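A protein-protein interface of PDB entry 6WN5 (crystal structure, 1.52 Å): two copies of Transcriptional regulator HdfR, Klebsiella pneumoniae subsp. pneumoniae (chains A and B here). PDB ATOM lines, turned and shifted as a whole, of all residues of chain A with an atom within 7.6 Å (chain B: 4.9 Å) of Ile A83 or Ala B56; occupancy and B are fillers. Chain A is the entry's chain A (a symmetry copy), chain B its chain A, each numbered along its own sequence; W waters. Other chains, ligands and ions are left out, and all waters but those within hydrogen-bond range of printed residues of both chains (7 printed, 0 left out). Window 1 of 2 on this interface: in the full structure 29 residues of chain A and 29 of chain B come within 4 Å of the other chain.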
ATOM      1  N   ILE A  52      22.168 -23.328  15.451  1.00  0.00           N
ATOM      2  CA  ILE A  52      21.186 -24.440  15.586  1.00  0.00           C
ATOM      3  C   ILE A  52      20.868 -24.552  17.065  1.00  0.00           C
ATOM      4  O   ILE A  52      21.818 -24.692  17.843  1.00  0.00           O
ATOM      5  CB  ILE A  52      21.764 -25.744  15.028  1.00  0.00           C
ATOM      6  CG1 ILE A  52      22.239 -25.567  13.585  1.00  0.00           C
ATOM      7  CG2 ILE A  52      20.756 -26.872  15.170  1.00  0.00           C
ATOM      8  CD1 ILE A  52      23.100 -26.684  13.079  1.00  0.00           C
ATOM      9  N   GLY A  53      19.600 -24.429  17.428  1.00  0.00           N
ATOM     10  CA  GLY A  53      19.189 -24.471  18.837  1.00  0.00           C
ATOM     11  C   GLY A  53      18.349 -25.684  19.148  1.00  0.00           C
ATOM     12  O   GLY A  53      17.524 -26.078  18.291  1.00  0.00           O
ATOM     13  N   ALA A  54      18.595 -26.272  20.305  1.00  0.00           N
ATOM     14  CA  ALA A  54      17.818 -27.426  20.767  1.00  0.00           C
ATOM     15  C   ALA A  54      18.038 -27.626  22.259  1.00  0.00           C
ATOM     16  O   ALA A  54      18.943 -27.024  22.831  1.00  0.00           O
ATOM     17  CB  ALA A  54      18.184 -28.686  20.015  1.00  0.00           C
ATOM     18  N   SER A  55      17.184 -28.468  22.842  1.00  0.00           N
ATOM     19  CA  SER A  55      17.320 -28.868  24.255  1.00  0.00           C
ATOM     20  C   SER A  55      18.628 -29.625  24.477  1.00  0.00           C
ATOM     21  O   SER A  55      19.203 -30.217  23.555  1.00  0.00           O
ATOM     22  CB  SER A  55      16.169 -29.720  24.655  1.00  0.00           C
ATOM     23  OG  SER A  55      16.230 -30.971  23.983  1.00  0.00           O
ATOM     24  N   ALA A  56      19.091 -29.639  25.721  1.00  0.00           N
ATOM     25  CA  ALA A  56      20.302 -30.399  26.069  1.00  0.00           C
ATOM     26  C   ALA A  56      20.162 -31.871  25.678  1.00  0.00           C
ATOM     27  O   ALA A  56      21.129 -32.452  25.145  1.00  0.00           O
ATOM     28  CB  ALA A  56      20.537 -30.271  27.555  1.00  0.00           C
ATOM     29  N   SER A  57      18.988 -32.453  25.906  1.00  0.00           N
ATOM     30  CA  SER A  57      18.808 -33.892  25.601  1.00  0.00           C
ATOM     31  C   SER A  57      18.852 -34.149  24.095  1.00  0.00           C
ATOM     32  O   SER A  57      19.357 -35.206  23.727  1.00  0.00           O
ATOM     33  CB  SER A  57      17.541 -34.390  26.204  1.00  0.00           C
ATOM     34  OG  SER A  57      16.474 -33.539  25.820  1.00  0.00           O
ATOM     35  N   TRP A  59      20.625 -32.519  21.880  1.00  0.00           N
ATOM     36  CA  TRP A  59      22.072 -32.494  21.535  1.00  0.00           C
ATOM     37  C   TRP A  59      22.765 -33.776  21.984  1.00  0.00           C
ATOM     38  O   TRP A  59      23.509 -34.370  21.177  1.00  0.00           O
ATOM     39  CB  TRP A  59      22.743 -31.251  22.120  1.00  0.00           C
ATOM     40  CG  TRP A  59      22.449 -30.012  21.360  1.00  0.00           C
ATOM     41  CD1 TRP A  59      21.656 -28.970  21.732  1.00  0.00           C
ATOM     42  CD2 TRP A  59      22.907 -29.708  20.034  1.00  0.00           C
ATOM     43  NE1 TRP A  59      21.608 -28.039  20.750  1.00  0.00           N
ATOM     44  CE2 TRP A  59      22.362 -28.456  19.682  1.00  0.00           C
ATOM     45  CE3 TRP A  59      23.691 -30.392  19.112  1.00  0.00           C
ATOM     46  CZ2 TRP A  59      22.595 -27.885  18.443  1.00  0.00           C
ATOM     47  CZ3 TRP A  59      23.945 -29.810  17.894  1.00  0.00           C
ATOM     48  CH2 TRP A  59      23.375 -28.591  17.559  1.00  0.00           C
ATOM     49  N   GLU A  60      22.516 -34.209  23.211  1.00  0.00           N
ATOM     50  CA  GLU A  60      23.200 -35.407  23.753  1.00  0.00           C
ATOM     51  C   GLU A  60      22.804 -36.677  22.993  1.00  0.00           C
ATOM     52  O   GLU A  60      23.667 -37.507  22.703  1.00  0.00           O
ATOM     53  CB  GLU A  60      22.802 -35.584  25.216  1.00  0.00           C
ATOM     54  CG  GLU A  60      23.391 -34.551  26.137  1.00  0.00           C
ATOM     55  CD  GLU A  60      22.696 -34.473  27.474  1.00  0.00           C
ATOM     56  OE1 GLU A  60      21.671 -35.176  27.651  1.00  0.00           O
ATOM     57  OE2 GLU A  60      23.169 -33.705  28.361  1.00  0.00           O
ATOM     58  N   ASN A  64      24.332 -34.197  18.235  1.00  0.00           N
ATOM     59  CA  ASN A  64      25.819 -34.089  18.220  1.00  0.00           C
ATOM     60  C   ASN A  64      26.341 -34.904  17.013  1.00  0.00           C
ATOM     61  O   ASN A  64      27.131 -34.368  16.206  1.00  0.00           O
ATOM     62  CB  ASN A  64      26.416 -34.508  19.575  1.00  0.00           C
ATOM     63  CG  ASN A  64      26.123 -33.578  20.753  1.00  0.00           C
ATOM     64  OD1 ASN A  64      25.580 -32.483  20.593  1.00  0.00           O
ATOM     65  ND2 ASN A  64      26.493 -33.990  21.962  1.00  0.00           N
ATOM     66  N   GLU A  80      27.076 -22.704  15.538  1.00  0.00           N
ATOM     67  CA  GLU A  80      26.828 -22.618  16.991  1.00  0.00           C
ATOM     68  C   GLU A  80      25.813 -23.686  17.366  1.00  0.00           C
ATOM     69  O   GLU A  80      24.752 -23.726  16.734  1.00  0.00           O
ATOM     70  CB  GLU A  80      26.296 -21.275  17.437  1.00  0.00           C
ATOM     71  CG  GLU A  80      26.004 -21.250  18.920  1.00  0.00           C
ATOM     72  CD  GLU A  80      25.343 -19.982  19.430  1.00  0.00           C
ATOM     73  OE1 GLU A  80      25.228 -19.020  18.627  1.00  0.00           O
ATOM     74  OE2 GLU A  80      24.929 -19.952  20.620  1.00  0.00           O
ATOM     75  N   ALA A  81      26.188 -24.565  18.287  1.00  0.00           N
ATOM     76  CA  ALA A  81      25.288 -25.581  18.854  1.00  0.00           C
ATOM     77  C   ALA A  81      24.698 -24.969  20.125  1.00  0.00           C
ATOM     78  O   ALA A  81      25.325 -25.070  21.194  1.00  0.00           O
ATOM     79  CB  ALA A  81      26.026 -26.869  19.119  1.00  0.00           C
ATOM     80  N   ARG A  82      23.558 -24.301  19.975  1.00  0.00           N
ATOM     81  CA  ARG A  82      22.977 -23.515  21.075  1.00  0.00           C
ATOM     82  C   ARG A  82      22.062 -24.410  21.897  1.00  0.00           C
ATOM     83  O   ARG A  82      21.218 -25.105  21.308  1.00  0.00           O
ATOM     84  CB  ARG A  82      22.190 -22.326  20.534  1.00  0.00           C
ATOM     85  CG  ARG A  82      21.721 -21.363  21.619  1.00  0.00           C
ATOM     86  CD  ARG A  82      21.097 -20.110  21.088  1.00  0.00           C
ATOM     87  NE  ARG A  82      22.041 -19.382  20.261  1.00  0.00           N
ATOM     88  CZ  ARG A  82      21.713 -18.367  19.457  1.00  0.00           C
ATOM     89  NH1 ARG A  82      20.453 -17.977  19.361  1.00  0.00           N
ATOM     90  NH2 ARG A  82      22.640 -17.793  18.713  1.00  0.00           N
ATOM     91  N   ILE A  83      22.254 -24.365  23.193  1.00  0.00           N
ATOM     92  CA  ILE A  83      21.421 -25.144  24.154  1.00  0.00           C
ATOM     93  C   ILE A  83      20.641 -24.109  24.941  1.00  0.00           C
ATOM     94  O   ILE A  83      21.271 -23.211  25.507  1.00  0.00           O
ATOM     95  CB  ILE A  83      22.292 -26.021  25.058  1.00  0.00           C
ATOM     96  CG1 ILE A  83      23.227 -26.923  24.261  1.00  0.00           C
ATOM     97  CG2 ILE A  83      21.422 -26.817  26.022  1.00  0.00           C
ATOM     98  CD1 ILE A  83      24.263 -27.653  25.108  1.00  0.00           C
ATOM     99  N   ALA A  84      19.318 -24.168  24.874  1.00  0.00           N
ATOM    100  CA  ALA A  84      18.494 -23.193  25.607  1.00  0.00           C
ATOM    101  C   ALA A  84      17.099 -23.772  25.773  1.00  0.00           C
ATOM    102  O   ALA A  84      16.779 -24.772  25.130  1.00  0.00           O
ATOM    103  CB  ALA A  84      18.448 -21.857  24.886  1.00  0.00           C
ATOM    104  N   GLN A  85      16.312 -23.134  26.641  1.00  0.00           N
ATOM    105  CA  GLN A  85      14.902 -23.515  26.895  1.00  0.00           C
ATOM    106  C   GLN A  85      14.054 -23.160  25.664  1.00  0.00           C
ATOM    107  O   GLN A  85      14.380 -22.196  24.954  1.00  0.00           O
ATOM    108  CB  GLN A  85      14.400 -22.810  28.157  1.00  0.00           C
ATOM    109  CG  GLN A  85      15.116 -23.245  29.427  1.00  0.00           C
ATOM    110  CD  GLN A  85      14.545 -22.600  30.666  1.00  0.00           C
ATOM    111  OE1 GLN A  85      14.520 -21.381  30.805  1.00  0.00           O
ATOM    112  NE2 GLN A  85      14.122 -23.426  31.599  1.00  0.00           N
ATOM    113  N   SER A  88      12.848 -19.466  24.973  1.00  0.00           N
ATOM    114  CA  SER A  88      13.953 -18.574  24.517  1.00  0.00           C
ATOM    115  C   SER A  88      14.283 -18.842  23.049  1.00  0.00           C
ATOM    116  O   SER A  88      14.407 -17.875  22.308  1.00  0.00           O
ATOM    117  CB  SER A  88      15.197 -18.707  25.351  1.00  0.00           C
ATOM    118  OG  SER A  88      14.985 -18.258  26.670  1.00  0.00           O
ATOM    119  N   LEU A  89      14.462 -20.111  22.661  1.00  0.00           N
ATOM    120  CA  LEU A  89      14.784 -20.423  21.245  1.00  0.00           C
ATOM    121  C   LEU A  89      13.674 -19.922  20.317  1.00  0.00           C
ATOM    122  O   LEU A  89      14.013 -19.403  19.265  1.00  0.00           O
ATOM    123  CB  LEU A  89      14.976 -21.934  21.068  1.00  0.00           C
ATOM    124  CG  LEU A  89      16.135 -22.544  21.854  1.00  0.00           C
ATOM    125  CD1 LEU A  89      16.089 -24.057  21.790  1.00  0.00           C
ATOM    126  CD2 LEU A  89      17.469 -22.026  21.355  1.00  0.00           C
ATOM    127  N   GLN A  92      13.970 -16.271  19.971  1.00  0.00           N
ATOM    128  CA  GLN A  92      15.183 -15.972  19.165  1.00  0.00           C
ATOM    129  C   GLN A  92      14.923 -16.192  17.661  1.00  0.00           C
ATOM    130  O   GLN A  92      15.486 -15.424  16.867  1.00  0.00           O
ATOM    131  CB  GLN A  92      16.356 -16.810  19.674  1.00  0.00           C
ATOM    132  CG  GLN A  92      16.886 -16.332  21.018  1.00  0.00           C
ATOM    133  CD  GLN A  92      17.784 -17.351  21.670  1.00  0.00           C
ATOM    134  OE1 GLN A  92      18.164 -18.337  21.054  1.00  0.00           O
ATOM    135  NE2 GLN A  92      18.137 -17.099  22.921  1.00  0.00           N
ATOM    136  N   LEU A  98      18.431 -16.580  16.133  1.00  0.00           N
ATOM    137  CA  LEU A  98      18.676 -18.042  15.982  1.00  0.00           C
ATOM    138  C   LEU A  98      18.293 -18.417  14.554  1.00  0.00           C
ATOM    139  O   LEU A  98      17.224 -17.970  14.096  1.00  0.00           O
ATOM    140  CB  LEU A  98      17.825 -18.826  16.981  1.00  0.00           C
ATOM    141  CG  LEU A  98      17.918 -20.354  16.871  1.00  0.00           C
ATOM    142  CD1 LEU A  98      19.301 -20.861  17.237  1.00  0.00           C
ATOM    143  CD2 LEU A  98      16.856 -21.013  17.734  1.00  0.00           C
ATOM    144  N   SER A 166      16.523 -31.403  31.882  1.00  0.00           N
ATOM    145  CA  SER A 166      16.449 -31.455  30.408  1.00  0.00           C
ATOM    146  C   SER A 166      17.670 -32.173  29.835  1.00  0.00           C
ATOM    147  O   SER A 166      17.762 -32.207  28.609  1.00  0.00           O
ATOM    148  CB  SER A 166      16.294 -30.094  29.803  1.00  0.00           C
ATOM    149  OG  SER A 166      17.340 -29.205  30.179  1.00  0.00           O
ATOM    150  N   SER A 167      18.570 -32.679  30.683  1.00  0.00           N
ATOM    151  CA  SER A 167      19.732 -33.452  30.187  1.00  0.00           C
ATOM    152  C   SER A 167      19.522 -34.960  30.382  1.00  0.00           C
ATOM    153  O   SER A 167      19.319 -35.394  31.529  1.00  0.00           O
ATOM    154  CB  SER A 167      20.996 -33.010  30.874  1.00  0.00           C
ATOM    155  OG  SER A 167      22.024 -33.963  30.662  1.00  0.00           O
ATOM    156  N   LEU A 170      22.415 -36.362  32.389  1.00  0.00           N
ATOM    157  CA  LEU A 170      22.291 -36.074  33.834  1.00  0.00           C
ATOM    158  C   LEU A 170      21.298 -37.057  34.457  1.00  0.00           C
ATOM    159  O   LEU A 170      21.592 -37.619  35.521  1.00  0.00           O
ATOM    160  CB  LEU A 170      21.839 -34.615  33.983  1.00  0.00           C
ATOM    161  CG  LEU A 170      21.946 -34.016  35.378  1.00  0.00           C
ATOM    162  CD1 LEU A 170      21.763 -32.510  35.335  1.00  0.00           C
ATOM    163  CD2 LEU A 170      20.949 -34.647  36.332  1.00  0.00           C
ATOM    164  N   ALA B  54      21.947 -23.670  35.994  1.00  0.00           N
ATOM    165  CA  ALA B  54      23.330 -23.454  35.558  1.00  0.00           C
ATOM    166  C   ALA B  54      23.460 -23.796  34.081  1.00  0.00           C
ATOM    167  O   ALA B  54      22.553 -24.396  33.509  1.00  0.00           O
ATOM    168  CB  ALA B  54      24.308 -24.276  36.368  1.00  0.00           C
ATOM    169  N   SER B  55      24.593 -23.387  33.510  1.00  0.00           N
ATOM    170  CA  SER B  55      24.937 -23.731  32.118  1.00  0.00           C
ATOM    171  C   SER B  55      25.094 -25.242  31.959  1.00  0.00           C
ATOM    172  O   SER B  55      25.372 -25.973  32.919  1.00  0.00           O
ATOM    173  CB  SER B  55      26.198 -23.048  31.723  1.00  0.00           C
ATOM    174  OG  SER B  55      27.295 -23.592  32.445  1.00  0.00           O
ATOM    175  N   ALA B  56      24.947 -25.718  30.729  1.00  0.00           N
ATOM    176  CA  ALA B  56      25.149 -27.148  30.442  1.00  0.00           C
ATOM    177  C   ALA B  56      26.537 -27.610  30.887  1.00  0.00           C
ATOM    178  O   ALA B  56      26.654 -28.708  31.468  1.00  0.00           O
ATOM    179  CB  ALA B  56      24.974 -27.367  28.959  1.00  0.00           C
ATOM    180  N   SER B  57      27.557 -26.789  30.653  1.00  0.00           N
ATOM    181  CA  SER B  57      28.935 -27.204  31.009  1.00  0.00           C
ATOM    182  C   SER B  57      29.112 -27.290  32.525  1.00  0.00           C
ATOM    183  O   SER B  57      29.857 -28.170  32.947  1.00  0.00           O
ATOM    184  CB  SER B  57      29.925 -26.278  30.394  1.00  0.00           C
ATOM    185  OG  SER B  57      29.580 -24.942  30.718  1.00  0.00           O
ATOM    186  N   LEU B  58      28.542 -26.368  33.311  1.00  0.00           N
ATOM    187  CA  LEU B  58      28.713 -26.552  34.777  1.00  0.00           C
ATOM    188  C   LEU B  58      28.022 -27.835  35.236  1.00  0.00           C
ATOM    189  O   LEU B  58      28.566 -28.528  36.098  1.00  0.00           O
ATOM    190  CB  LEU B  58      28.178 -25.331  35.539  1.00  0.00           C
ATOM    191  CG  LEU B  58      29.027 -24.069  35.436  1.00  0.00           C
ATOM    192  CD1 LEU B  58      28.459 -22.983  36.329  1.00  0.00           C
ATOM    193  CD2 LEU B  58      30.480 -24.338  35.798  1.00  0.00           C
ATOM    194  N   TRP B  59      26.840 -28.147  34.718  1.00  0.00           N
ATOM    195  CA  TRP B  59      26.212 -29.442  35.099  1.00  0.00           C
ATOM    196  C   TRP B  59      27.105 -30.618  34.719  1.00  0.00           C
ATOM    197  O   TRP B  59      27.320 -31.507  35.568  1.00  0.00           O
ATOM    198  CB  TRP B  59      24.818 -29.565  34.483  1.00  0.00           C
ATOM    199  CG  TRP B  59      23.792 -28.758  35.186  1.00  0.00           C
ATOM    200  CD1 TRP B  59      23.180 -27.622  34.753  1.00  0.00           C
ATOM    201  CD2 TRP B  59      23.293 -28.998  36.509  1.00  0.00           C
ATOM    202  NE1 TRP B  59      22.326 -27.157  35.695  1.00  0.00           N
ATOM    203  CE2 TRP B  59      22.368 -27.973  36.797  1.00  0.00           C
ATOM    204  CE3 TRP B  59      23.569 -29.957  37.477  1.00  0.00           C
ATOM    205  CZ2 TRP B  59      21.720 -27.902  38.019  1.00  0.00           C
ATOM    206  CZ3 TRP B  59      22.903 -29.901  38.678  1.00  0.00           C
ATOM    207  CH2 TRP B  59      22.019 -28.868  38.950  1.00  0.00           C
ATOM    208  N   GLU B  60      27.635 -30.617  33.503  1.00  0.00           N
ATOM    209  CA  GLU B  60      28.457 -31.754  33.027  1.00  0.00           C
ATOM    210  C   GLU B  60      29.758 -31.885  33.826  1.00  0.00           C
ATOM    211  O   GLU B  60      30.151 -33.001  34.171  1.00  0.00           O
ATOM    212  CB  GLU B  60      28.819 -31.522  31.563  1.00  0.00           C
ATOM    213  CG  GLU B  60      27.660 -31.670  30.616  1.00  0.00           C
ATOM    214  CD  GLU B  60      27.909 -31.057  29.260  1.00  0.00           C
ATOM    215  OE1 GLU B  60      28.976 -30.420  29.085  1.00  0.00           O
ATOM    216  OE2 GLU B  60      27.038 -31.208  28.357  1.00  0.00           O
ATOM    217  N   ILE B  83      18.776 -26.332  33.126  1.00  0.00           N
ATOM    218  CA  ILE B  83      19.853 -25.932  32.177  1.00  0.00           C
ATOM    219  C   ILE B  83      19.252 -24.827  31.330  1.00  0.00           C
ATOM    220  O   ILE B  83      18.188 -25.054  30.744  1.00  0.00           O
ATOM    221  CB  ILE B  83      20.316 -27.121  31.330  1.00  0.00           C
ATOM    222  CG1 ILE B  83      20.733 -28.312  32.186  1.00  0.00           C
ATOM    223  CG2 ILE B  83      21.424 -26.694  30.376  1.00  0.00           C
ATOM    224  CD1 ILE B  83      20.992 -29.589  31.395  1.00  0.00           C
ATOM    225  N   GLN B  85      20.191 -20.550  29.483  1.00  0.00           N
ATOM    226  CA  GLN B  85      21.126 -19.433  29.208  1.00  0.00           C
ATOM    227  C   GLN B  85      21.120 -18.466  30.401  1.00  0.00           C
ATOM    228  O   GLN B  85      20.090 -18.339  31.081  1.00  0.00           O
ATOM    229  CB  GLN B  85      20.723 -18.736  27.906  1.00  0.00           C
ATOM    230  CG  GLN B  85      20.856 -19.617  26.673  1.00  0.00           C
ATOM    231  CD  GLN B  85      20.535 -18.881  25.396  1.00  0.00           C
ATOM    232  OE1 GLN B  85      19.439 -18.362  25.208  1.00  0.00           O
ATOM    233  NE2 GLN B  85      21.486 -18.872  24.486  1.00  0.00           N
ATOM    234  N   THR B 165      29.656 -23.429  21.582  1.00  0.00           N
ATOM    235  CA  THR B 165      28.576 -24.142  22.315  1.00  0.00           C
ATOM    236  C   THR B 165      28.713 -23.851  23.796  1.00  0.00           C
ATOM    237  O   THR B 165      29.720 -23.244  24.205  1.00  0.00           O
ATOM    238  CB  THR B 165      28.581 -25.640  21.985  1.00  0.00           C
ATOM    239  OG1 THR B 165      27.407 -26.233  22.555  1.00  0.00           O
ATOM    240  CG2 THR B 165      29.812 -26.360  22.473  1.00  0.00           C
ATOM    241  N   SER B 166      27.769 -24.348  24.579  1.00  0.00           N
ATOM    242  CA  SER B 166      27.809 -24.243  26.051  1.00  0.00           C
ATOM    243  C   SER B 166      27.946 -25.628  26.683  1.00  0.00           C
ATOM    244  O   SER B 166      27.908 -25.678  27.912  1.00  0.00           O
ATOM    245  CB  SER B 166      26.618 -23.519  26.598  1.00  0.00           C
ATOM    246  OG  SER B 166      25.387 -24.121  26.214  1.00  0.00           O
ATOM    247  N   SER B 167      28.057 -26.690  25.879  1.00  0.00           N
ATOM    248  CA  SER B 167      28.270 -28.046  26.435  1.00  0.00           C
ATOM    249  C   SER B 167      29.735 -28.482  26.295  1.00  0.00           C
ATOM    250  O   SER B 167      30.243 -28.520  25.160  1.00  0.00           O
ATOM    251  CB  SER B 167      27.363 -29.043  25.763  1.00  0.00           C
ATOM    252  OG  SER B 167      27.803 -30.362  26.039  1.00  0.00           O
HETATM  253  O   HOH W   1      21.797 -16.829  22.581  1.00  0.00           O
HETATM  254  O   HOH W   2      24.322 -31.246  28.325  1.00  0.00           O
HETATM  255  O   HOH W   3      24.452 -22.638  24.155  1.00  0.00           O
HETATM  256  O   HOH W   4      16.322 -27.663  32.153  1.00  0.00           O
HETATM  257  O   HOH W   5      25.919 -32.163  24.692  1.00  0.00           O
HETATM  258  O   HOH W   6      18.781 -25.344  28.093  1.00  0.00           O
HETATM  259  O   HOH W   7      26.118 -34.029  28.403  1.00  0.00           O
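OE1 of Gln B85 is in hydrogen-bond range of NE2 of Gln A92 (2.9 Å). The backbone carbonyl oxygen of Ala A81 sits at hydrogen-bond distance from the side-chain hydroxyl of Thr B165 (2.7 Å).
Gly A53 touches none of the printed residues of chain B. Ser A57 touches none of the printed residues of chain B. Printed residues of chain B within 4 Å of Ala A81: Thr B165. Printed residues of chain B within 4 Å of Ile A83: Ala B56, Gln B85, Ser B166 and Ser B167. Of the printed residues of chain B, Ala A84 touches Gln B85. Printed residues of chain B within 4 Å of Ser A167: Ile B83 (3.5 Å). Of chain A, only Ile A83 (3.9 Å) comes within 4 Å of Ala B56. Printed residues of chain A within 4 Å of Ile B83: Ala A56, Gln A85, Ser A166 and Ser A167. Printed residues of chain A within 4 Å of Gln B85: Arg A82 (3.6 Å), Ile A83 (3.8 Å), Ala A84 (3.6 Å) and Gln A92 (2.9 Å). The nearest printed residue of chain B that does not touch Ile A83 is Thr B165 (4.3 Å). The nearest residue of chain A that does not touch Ala B56 is Ala A56 (5.5 Å).
Water W3 lies within hydrogen-bond range of the side-chain hydroxyl of Ser B166 and the backbone NH of Ile A83. Water W4 bridges the side-chain hydroxyl (OG) of Ser A166 and the backbone NH (N) of Ile B83. Water W2 lies within hydrogen-bond range of the side-chain carboxylate of Glu B60 and the side-chain carboxylate of Glu A60. Water W6 lies within hydrogen-bond range of the backbone carbonyl oxygen of Ile B83 (2.7 Å) and the backbone NH of Ala A84 (3.5 Å). Water W1 lies within hydrogen-bond range of NE2 of Gln B85 (2.8 Å) and NE of Arg A82 (3.5 Å). Water W5 lies within hydrogen-bond range of OG of Ser B167 (2.9 Å) and ND2 of Asn A64 (3.3 Å).
Ala A56 touches Ile B83, and with the chains exchanged Ile A83 touches Ala B56. Ile A83 touches Gln B85, and with the chains exchanged Gln A85 touches Ile B83. Ile A83 touches Ser B166, and with the chains exchanged Ser A166 touches Ile B83. Ile A83 touches Ser B167, and with the chains exchanged Ser A167 touches Ile B83. 10 positions are printed for both chains. Of the 13 pairs that touch across the chains among the printed residues, 8 have their exchanged pair printed and touching as well.
Among the printed residues, pairs that only touch across the chains: Ala A56 with Ile B83, Arg A82 with Gln B85, Ile A83 with Ala B56, Ile A83 with Gln B85, Ile A83 with Ser B166, Ile A83 with Ser B167, Ala A84 with Gln B85, Gln A85 with Ile B83, Ser A166 with Ile B83, Ser A167 with Ile B83 and Leu A170 with Trp B59.
Of the 12 printed residues of chain B, 7 touch a printed residue of chain A. Hydrophobic or aromatic side chains of chain B that line the printed part of chain A: Ala B56, Trp B59 and Ile B83. Along chain B the printed residues that touch a printed residue of chain A span positions 56 to 167. Of the 22 printed residues of chain A, 10 touch a printed residue of chain B. Printed residues of chain A that touch a printed residue of chain B: Ala A56, Ala A81, Arg A82, Ile A83, Ala A84, Gln A85, Gln A92, Ser A166, Ser A167 and Leu A170. Among the printed residues, 13 pairs touch across the chains. Among the printed residues, no Asp or Glu carboxylate lies within 4 Å of a Lys or Arg side-chain nitrogen of the other chain.
NH1 of Arg A82 sits at hydrogen-bond distance from OE1 of Gln A92 (2.9 Å). O of Ile A52 lies within hydrogen-bond range of N of Arg A82, 2.8 Å away. The backbone NH of Ala A54 lies within hydrogen-bond range of the backbone carbonyl oxygen of Arg A82 (3.0 Å). The backbone carbonyl oxygen of Ser A166 is in hydrogen-bond range of the backbone NH of Ser A57. NH2 of Arg A82 is in salt-bridge range of OE1 of Glu A80 (2.9 Å). The side-chain hydroxyl (OG1) of Thr B165 is in hydrogen-bond range of the backbone NH (N) of Ser B167 (3.4 Å).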
